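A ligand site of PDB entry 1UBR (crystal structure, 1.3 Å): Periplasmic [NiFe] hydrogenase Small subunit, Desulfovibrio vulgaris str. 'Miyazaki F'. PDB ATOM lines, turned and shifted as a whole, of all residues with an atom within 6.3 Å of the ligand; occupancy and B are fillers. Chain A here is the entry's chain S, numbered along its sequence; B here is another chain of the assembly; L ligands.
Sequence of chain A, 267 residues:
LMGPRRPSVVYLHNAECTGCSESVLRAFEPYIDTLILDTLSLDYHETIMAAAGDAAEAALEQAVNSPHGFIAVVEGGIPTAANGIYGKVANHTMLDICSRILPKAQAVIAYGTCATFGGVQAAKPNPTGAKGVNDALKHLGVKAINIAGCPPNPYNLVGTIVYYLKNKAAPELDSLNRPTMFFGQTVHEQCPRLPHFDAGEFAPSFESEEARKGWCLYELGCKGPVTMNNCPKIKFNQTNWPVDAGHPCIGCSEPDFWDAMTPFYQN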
ATOM      1  N   ALA A  15     -11.005   8.173   4.872  1.00  0.00           N
ATOM      2  CA  ALA A  15     -11.834   7.961   3.693  1.00  0.00           C
ATOM      3  C   ALA A  15     -12.491   6.612   3.927  1.00  0.00           C
ATOM      4  O   ALA A  15     -11.869   5.581   3.782  1.00  0.00           O
ATOM      5  CB  ALA A  15     -10.994   7.965   2.412  1.00  0.00           C
ATOM      6  N   GLU A  16     -13.773   6.630   4.316  1.00  0.00           N
ATOM      7  CA  GLU A  16     -14.463   5.484   4.824  1.00  0.00           C
ATOM      8  C   GLU A  16     -15.954   5.620   4.567  1.00  0.00           C
ATOM      9  O   GLU A  16     -16.432   6.693   4.214  1.00  0.00           O
ATOM     10  CB  GLU A  16     -14.168   5.313   6.346  1.00  0.00           C
ATOM     11  CG  GLU A  16     -14.304   6.599   7.156  1.00  0.00           C
ATOM     12  CD  GLU A  16     -15.695   6.997   7.574  1.00  0.00           C
ATOM     13  OE1 GLU A  16     -16.508   6.109   7.939  1.00  0.00           O
ATOM     14  OE2 GLU A  16     -15.974   8.217   7.605  1.00  0.00           O
ATOM     15  N   CYS A  17     -16.679   4.488   4.659  1.00  0.00           N
ATOM     16  CA  CYS A  17     -18.096   4.415   4.428  1.00  0.00           C
ATOM     17  C   CYS A  17     -18.865   4.280   5.728  1.00  0.00           C
ATOM     18  O   CYS A  17     -20.097   4.265   5.702  1.00  0.00           O
ATOM     19  CB  CYS A  17     -18.445   3.246   3.503  1.00  0.00           C
ATOM     20  SG  CYS A  17     -18.485   1.623   4.329  1.00  0.00           S
ATOM     21  N   THR A  18     -18.171   4.147   6.843  1.00  0.00           N
ATOM     22  CA  THR A  18     -18.735   4.030   8.199  1.00  0.00           C
ATOM     23  C   THR A  18     -19.289   2.638   8.459  1.00  0.00           C
ATOM     24  O   THR A  18     -19.784   2.338   9.544  1.00  0.00           O
ATOM     25  CB  THR A  18     -19.710   5.170   8.509  1.00  0.00           C
ATOM     26  OG1 THR A  18     -19.074   6.400   8.080  1.00  0.00           O
ATOM     27  CG2 THR A  18     -20.023   5.292   9.997  1.00  0.00           C
ATOM     28  N   GLY A  19     -19.096   1.708   7.515  1.00  0.00           N
ATOM     29  CA  GLY A  19     -19.446   0.307   7.726  1.00  0.00           C
ATOM     30  C   GLY A  19     -18.592  -0.296   8.807  1.00  0.00           C
ATOM     31  O   GLY A  19     -19.062  -1.179   9.561  1.00  0.00           O
ATOM     32  N   CYS A  20     -17.320   0.145   8.910  1.00  0.00           N
ATOM     33  CA  CYS A  20     -16.519  -0.437  10.000  1.00  0.00           C
ATOM     34  C   CYS A  20     -17.008   0.072  11.328  1.00  0.00           C
ATOM     35  O   CYS A  20     -17.106  -0.698  12.292  1.00  0.00           O
ATOM     36  CB  CYS A  20     -15.032  -0.129   9.734  1.00  0.00           C
ATOM     37  SG  CYS A  20     -14.305  -1.080   8.411  1.00  0.00           S
ATOM     38  N   SER A  21     -17.317   1.368  11.494  1.00  0.00           N
ATOM     39  CA  SER A  21     -17.924   1.826  12.730  1.00  0.00           C
ATOM     40  C   SER A  21     -19.190   1.057  13.051  1.00  0.00           C
ATOM     41  O   SER A  21     -19.406   0.682  14.214  1.00  0.00           O
ATOM     42  CB  SER A  21     -18.369   3.307  12.630  1.00  0.00           C
ATOM     43  OG  SER A  21     -17.207   4.141  12.687  1.00  0.00           O
ATOM     44  N   GLU A  75     -10.324   4.032  11.005  1.00  0.00           N
ATOM     45  CA  GLU A  75     -11.198   3.533   9.936  1.00  0.00           C
ATOM     46  C   GLU A  75     -10.979   4.366   8.693  1.00  0.00           C
ATOM     47  O   GLU A  75     -10.953   5.603   8.835  1.00  0.00           O
ATOM     48  CB  GLU A  75     -12.660   3.578  10.440  1.00  0.00           C
ATOM     49  CG  GLU A  75     -13.743   3.245   9.409  1.00  0.00           C
ATOM     50  CD  GLU A  75     -15.146   3.268  10.022  1.00  0.00           C
ATOM     51  OE1 GLU A  75     -16.079   2.943   9.250  1.00  0.00           O
ATOM     52  OE2 GLU A  75     -15.236   3.622  11.223  1.00  0.00           O
ATOM     53  N   GLY A  76     -10.820   3.735   7.535  1.00  0.00           N
ATOM     54  CA  GLY A  76     -10.694   4.432   6.275  1.00  0.00           C
ATOM     55  C   GLY A  76      -9.246   4.596   5.800  1.00  0.00           C
ATOM     56  O   GLY A  76      -8.289   4.659   6.583  1.00  0.00           O
ATOM     57  N   GLY A  77      -9.113   4.724   4.480  1.00  0.00           N
ATOM     58  CA  GLY A  77      -7.837   4.948   3.825  1.00  0.00           C
ATOM     59  C   GLY A  77      -7.464   6.416   3.921  1.00  0.00           C
ATOM     60  O   GLY A  77      -8.332   7.246   4.161  1.00  0.00           O
ATOM     61  N   TYR A 111      -8.513  -0.551  11.302  1.00  0.00           N
ATOM     62  CA  TYR A 111      -9.686  -1.420  11.314  1.00  0.00           C
ATOM     63  C   TYR A 111     -10.429  -1.284  10.000  1.00  0.00           C
ATOM     64  O   TYR A 111     -10.887  -0.180   9.683  1.00  0.00           O
ATOM     65  CB  TYR A 111     -10.571  -1.040  12.511  1.00  0.00           C
ATOM     66  CG  TYR A 111     -11.774  -1.955  12.678  1.00  0.00           C
ATOM     67  CD1 TYR A 111     -11.604  -3.342  12.901  1.00  0.00           C
ATOM     68  CD2 TYR A 111     -13.061  -1.469  12.585  1.00  0.00           C
ATOM     69  CE1 TYR A 111     -12.682  -4.216  13.055  1.00  0.00           C
ATOM     70  CE2 TYR A 111     -14.118  -2.322  12.739  1.00  0.00           C
ATOM     71  CZ  TYR A 111     -13.975  -3.677  12.959  1.00  0.00           C
ATOM     72  OH  TYR A 111     -15.033  -4.542  13.108  1.00  0.00           O
ATOM     73  N   GLY A 112     -10.488  -2.392   9.250  1.00  0.00           N
ATOM     74  CA  GLY A 112     -11.130  -2.496   7.964  1.00  0.00           C
ATOM     75  C   GLY A 112     -10.084  -2.423   6.840  1.00  0.00           C
ATOM     76  O   GLY A 112      -9.053  -1.758   6.965  1.00  0.00           O
ATOM     77  N   THR A 113     -10.409  -3.112   5.741  1.00  0.00           N
ATOM     78  CA  THR A 113      -9.510  -3.134   4.599  1.00  0.00           C
ATOM     79  C   THR A 113      -9.126  -1.758   4.086  1.00  0.00           C
ATOM     80  O   THR A 113      -8.023  -1.608   3.550  1.00  0.00           O
ATOM     81  CB  THR A 113     -10.190  -4.003   3.493  1.00  0.00           C
ATOM     82  OG1 THR A 113     -10.255  -5.333   4.065  1.00  0.00           O
ATOM     83  CG2 THR A 113      -9.445  -4.039   2.165  1.00  0.00           C
ATOM     84  N   CYS A 114      -9.970  -0.775   4.190  1.00  0.00           N
ATOM     85  CA  CYS A 114      -9.525   0.563   3.766  1.00  0.00           C
ATOM     86  C   CYS A 114      -8.377   1.059   4.616  1.00  0.00           C
ATOM     87  O   CYS A 114      -7.355   1.528   4.087  1.00  0.00           O
ATOM     88  CB  CYS A 114     -10.688   1.577   3.887  1.00  0.00           C
ATOM     89  SG  CYS A 114     -12.102   1.284   2.752  1.00  0.00           S
ATOM     90  N   ALA A 115      -8.547   1.009   5.954  1.00  0.00           N
ATOM     91  CA  ALA A 115      -7.430   1.447   6.779  1.00  0.00           C
ATOM     92  C   ALA A 115      -6.248   0.515   6.663  1.00  0.00           C
ATOM     93  O   ALA A 115      -5.083   0.926   6.787  1.00  0.00           O
ATOM     94  CB  ALA A 115      -7.870   1.509   8.253  1.00  0.00           C
ATOM     95  N   GLY A 119      -8.198  -0.058   0.397  1.00  0.00           N
ATOM     96  CA  GLY A 119      -9.636  -0.269   0.263  1.00  0.00           C
ATOM     97  C   GLY A 119     -10.261   0.303  -1.005  1.00  0.00           C
ATOM     98  O   GLY A 119      -9.629   0.520  -2.023  1.00  0.00           O
ATOM     99  N   VAL A 120     -11.585   0.549  -0.914  1.00  0.00           N
ATOM    100  CA  VAL A 120     -12.374   0.735  -2.120  1.00  0.00           C
ATOM    101  C   VAL A 120     -11.909   1.985  -2.839  1.00  0.00           C
ATOM    102  O   VAL A 120     -11.854   1.962  -4.084  1.00  0.00           O
ATOM    103  CB  VAL A 120     -13.888   0.760  -1.811  1.00  0.00           C
ATOM    104  CG1 VAL A 120     -14.300   1.989  -1.013  1.00  0.00           C
ATOM    105  CG2 VAL A 120     -14.727   0.657  -3.090  1.00  0.00           C
ATOM    106  N   GLN A 121     -11.581   3.072  -2.145  1.00  0.00           N
ATOM    107  CA  GLN A 121     -11.185   4.263  -2.903  1.00  0.00           C
ATOM    108  C   GLN A 121      -9.782   4.110  -3.438  1.00  0.00           C
ATOM    109  O   GLN A 121      -9.363   4.928  -4.293  1.00  0.00           O
ATOM    110  CB  GLN A 121     -11.282   5.527  -2.039  1.00  0.00           C
ATOM    111  CG  GLN A 121     -10.518   5.452  -0.709  1.00  0.00           C
ATOM    112  CD  GLN A 121     -11.304   4.774   0.369  1.00  0.00           C
ATOM    113  OE1 GLN A 121     -12.490   5.017   0.573  1.00  0.00           O
ATOM    114  NE2 GLN A 121     -10.721   3.857   1.109  1.00  0.00           N
ATOM    115  N   GLY A 149     -10.992  -6.802   6.399  1.00  0.00           N
ATOM    116  CA  GLY A 149     -12.367  -7.167   6.076  1.00  0.00           C
ATOM    117  C   GLY A 149     -13.142  -5.908   5.712  1.00  0.00           C
ATOM    118  O   GLY A 149     -12.748  -4.809   6.139  1.00  0.00           O
ATOM    119  N   CYS A 150     -14.273  -6.084   5.031  1.00  0.00           N
ATOM    120  CA  CYS A 150     -14.997  -4.920   4.503  1.00  0.00           C
ATOM    121  C   CYS A 150     -16.482  -5.015   4.786  1.00  0.00           C
ATOM    122  O   CYS A 150     -17.306  -5.223   3.883  1.00  0.00           O
ATOM    123  CB  CYS A 150     -14.683  -4.825   3.002  1.00  0.00           C
ATOM    124  SG  CYS A 150     -15.165  -3.254   2.242  1.00  0.00           S
ATOM    125  N   PRO A 151     -16.881  -4.846   6.047  1.00  0.00           N
ATOM    126  CA  PRO A 151     -16.022  -4.625   7.201  1.00  0.00           C
ATOM    127  C   PRO A 151     -15.564  -5.910   7.897  1.00  0.00           C
ATOM    128  O   PRO A 151     -16.039  -7.013   7.579  1.00  0.00           O
ATOM    129  CB  PRO A 151     -16.966  -3.882   8.162  1.00  0.00           C
ATOM    130  CG  PRO A 151     -18.298  -4.546   7.858  1.00  0.00           C
ATOM    131  CD  PRO A 151     -18.346  -4.824   6.380  1.00  0.00           C
ATOM    132  N   PRO A 152     -14.611  -5.812   8.783  1.00  0.00           N
ATOM    133  CA  PRO A 152     -14.106  -6.982   9.512  1.00  0.00           C
ATOM    134  C   PRO A 152     -15.185  -7.514  10.412  1.00  0.00           C
ATOM    135  O   PRO A 152     -16.194  -6.849  10.712  1.00  0.00           O
ATOM    136  CB  PRO A 152     -12.967  -6.434  10.404  1.00  0.00           C
ATOM    137  CG  PRO A 152     -12.598  -5.112   9.758  1.00  0.00           C
ATOM    138  CD  PRO A 152     -13.928  -4.569   9.254  1.00  0.00           C
ATOM    139  N   TRP A 258     -10.279  -5.283  -4.467  1.00  0.00           N
ATOM    140  CA  TRP A 258     -11.166  -4.740  -5.530  1.00  0.00           C
ATOM    141  C   TRP A 258     -10.598  -4.971  -6.932  1.00  0.00           C
ATOM    142  O   TRP A 258     -11.358  -5.079  -7.897  1.00  0.00           O
ATOM    143  CB  TRP A 258     -11.313  -3.241  -5.272  1.00  0.00           C
ATOM    144  CG  TRP A 258     -11.980  -3.011  -3.939  1.00  0.00           C
ATOM    145  CD1 TRP A 258     -11.394  -2.609  -2.783  1.00  0.00           C
ATOM    146  CD2 TRP A 258     -13.364  -3.200  -3.652  1.00  0.00           C
ATOM    147  NE1 TRP A 258     -12.323  -2.523  -1.780  1.00  0.00           N
ATOM    148  CE2 TRP A 258     -13.546  -2.881  -2.302  1.00  0.00           C
ATOM    149  CE3 TRP A 258     -14.456  -3.602  -4.434  1.00  0.00           C
ATOM    150  CZ2 TRP A 258     -14.796  -2.937  -1.634  1.00  0.00           C
ATOM    151  CZ3 TRP A 258     -15.706  -3.667  -3.800  1.00  0.00           C
ATOM    152  CH2 TRP A 258     -15.857  -3.349  -2.431  1.00  0.00           C
ATOM    153  N   ARG B  41     -14.217  10.326  -2.641  1.00  0.00           N
ATOM    154  CA  ARG B  41     -13.627   9.043  -2.932  1.00  0.00           C
ATOM    155  C   ARG B  41     -13.602   8.734  -4.414  1.00  0.00           C
ATOM    156  O   ARG B  41     -12.595   8.162  -4.888  1.00  0.00           O
ATOM    157  CB  ARG B  41     -14.364   7.910  -2.187  1.00  0.00           C
ATOM    158  CG  ARG B  41     -14.045   7.964  -0.697  1.00  0.00           C
ATOM    159  CD  ARG B  41     -14.792   7.002   0.193  1.00  0.00           C
ATOM    160  NE  ARG B  41     -16.203   7.280   0.052  1.00  0.00           N
ATOM    161  CZ  ARG B  41     -17.206   6.451   0.183  1.00  0.00           C
ATOM    162  NH1 ARG B  41     -16.998   5.191   0.546  1.00  0.00           N
ATOM    163  NH2 ARG B  41     -18.443   6.852  -0.026  1.00  0.00           N
ATOM    164  N   ARG B  61     -20.233  -0.105  -0.922  1.00  0.00           N
ATOM    165  CA  ARG B  61     -19.260   0.583  -0.047  1.00  0.00           C
ATOM    166  C   ARG B  61     -19.332   2.102  -0.187  1.00  0.00           C
ATOM    167  O   ARG B  61     -18.501   2.819   0.374  1.00  0.00           O
ATOM    168  CB  ARG B  61     -17.849   0.095  -0.316  1.00  0.00           C
ATOM    169  CG  ARG B  61     -17.570  -1.230   0.375  1.00  0.00           C
ATOM    170  CD  ARG B  61     -18.416  -2.395  -0.132  1.00  0.00           C
ATOM    171  NE  ARG B  61     -18.002  -3.582   0.628  1.00  0.00           N
ATOM    172  CZ  ARG B  61     -18.535  -4.805   0.421  1.00  0.00           C
ATOM    173  NH1 ARG B  61     -19.432  -4.987  -0.543  1.00  0.00           N
ATOM    174  NH2 ARG B  61     -18.168  -5.806   1.193  1.00  0.00           N
ATOM    175  N   GLY B  64     -21.900   2.356   4.747  1.00  0.00           N
ATOM    176  CA  GLY B  64     -22.174   1.256   5.651  1.00  0.00           C
ATOM    177  C   GLY B  64     -23.214   1.562   6.701  1.00  0.00           C
ATOM    178  O   GLY B  64     -23.549   0.669   7.452  1.00  0.00           O
ATOM    179  N   PRO B 216     -22.738  -5.205   8.791  1.00  0.00           N
ATOM    180  CA  PRO B 216     -22.946  -4.478   7.531  1.00  0.00           C
ATOM    181  C   PRO B 216     -22.477  -5.193   6.261  1.00  0.00           C
ATOM    182  O   PRO B 216     -21.614  -6.108   6.332  1.00  0.00           O
ATOM    183  CB  PRO B 216     -22.050  -3.200   7.695  1.00  0.00           C
ATOM    184  CG  PRO B 216     -21.880  -3.085   9.191  1.00  0.00           C
ATOM    185  CD  PRO B 216     -21.734  -4.541   9.647  1.00  0.00           C
ATOM    186  N   HIS B 217     -23.021  -4.689   5.144  1.00  0.00           N
ATOM    187  CA  HIS B 217     -22.675  -4.989   3.756  1.00  0.00           C
ATOM    188  C   HIS B 217     -23.139  -6.402   3.431  1.00  0.00           C
ATOM    189  O   HIS B 217     -22.422  -7.411   3.533  1.00  0.00           O
ATOM    190  CB  HIS B 217     -21.180  -4.783   3.479  1.00  0.00           C
ATOM    191  CG  HIS B 217     -20.868  -3.300   3.444  1.00  0.00           C
ATOM    192  ND1 HIS B 217     -19.674  -2.700   3.515  1.00  0.00           N
ATOM    193  CD2 HIS B 217     -21.821  -2.304   3.330  1.00  0.00           C
ATOM    194  CE1 HIS B 217     -19.848  -1.358   3.444  1.00  0.00           C
ATOM    195  NE2 HIS B 217     -21.156  -1.123   3.328  1.00  0.00           N
HETATM  196 FE1  LIG L   1     -16.389   0.745   4.466  1.00  0.00          FE
HETATM  197 FE2  LIG L   1     -13.768   0.615   4.069  1.00  0.00          FE
HETATM  198 FE3  LIG L   1     -15.213  -1.553   3.803  1.00  0.00          FE
HETATM  199 FE4  LIG L   1     -14.861  -0.517   6.284  1.00  0.00          FE
HETATM  200  S1  LIG L   1     -13.239  -1.427   4.979  1.00  0.00           S
HETATM  201  S2  LIG L   1     -16.756  -1.336   5.371  1.00  0.00           S
HETATM  202  S3  LIG L   1     -14.757   1.749   5.789  1.00  0.00           S
HETATM  203  S4  LIG L   1     -15.385   0.354   2.485  1.00  0.00           S
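SG of Cys 17 lies close to N of Gly 19, at 3.2 Å. The backbone NH of Cys 20 lies within hydrogen-bond range of the side-chain carboxylate of Glu 75, 3.1 Å away. The side-chain hydroxyl (OG1) of Thr 18 lies within hydrogen-bond range of the side-chain carboxylate (OE1) of Glu 16 (2.6 Å). The side-chain sulfur of Cys 114 sits close to the backbone NH of Val 120, at 3.8 Å. The backbone NH (N) of Gly 64 of chain B lies within hydrogen-bond range of the backbone carbonyl oxygen (O) of Cys 17 (2.8 Å). NH2 of Arg 61 of chain B sits at hydrogen-bond distance from O of Cys 150, at 2.9 Å. The side-chain carboxylate (OE1) of Glu 75 sits close to the backbone NH (N) of Thr 18 (3.4 Å). SG of Cys 114 lies close to NE2 of Gln 121 (3.4 Å).
A sulfur (S1) of the ligand lies close to the backbone NH of Cys 114, at 3.4 Å. SG of Cys 20 binds FE4 of the ligand. An iron atom (FE2) of the ligand is bound by the side-chain sulfur (SG) of Cys 114 (2.2 Å). SG of Cys 150 is bound to FE3 of the ligand (2.3 Å). SG of Cys 17 binds FE1 of the ligand, at 2.3 Å. The backbone NH (N) of Thr 113 lies close to a sulfur (S1) of the ligand (3.4 Å). S2 of the ligand sits close to ND1 of His 217 of chain B (3.7 Å). S3 of the ligand sits close to N of Cys 17, at 3.5 Å.
The backbone carbonyl oxygen (O) of Gly 149 sits close to a sulfur (S1) of the ligand. A sulfur (S2) of the ligand lies close to the backbone nitrogen of Pro 151 (3.6 Å). Glu 16 touches the ligand (CB to S3, 3.7 Å). CA of Gly 19 touches S2 of the ligand, 3.9 Å away. Glu 75 touches the ligand (OE1 to S3, 3.9 Å). Gly 112 touches the ligand. Arg 61 of chain B touches the ligand. Hydrophobic or aromatic side chains that line the ligand: Pro 151 and His 217 of chain B.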
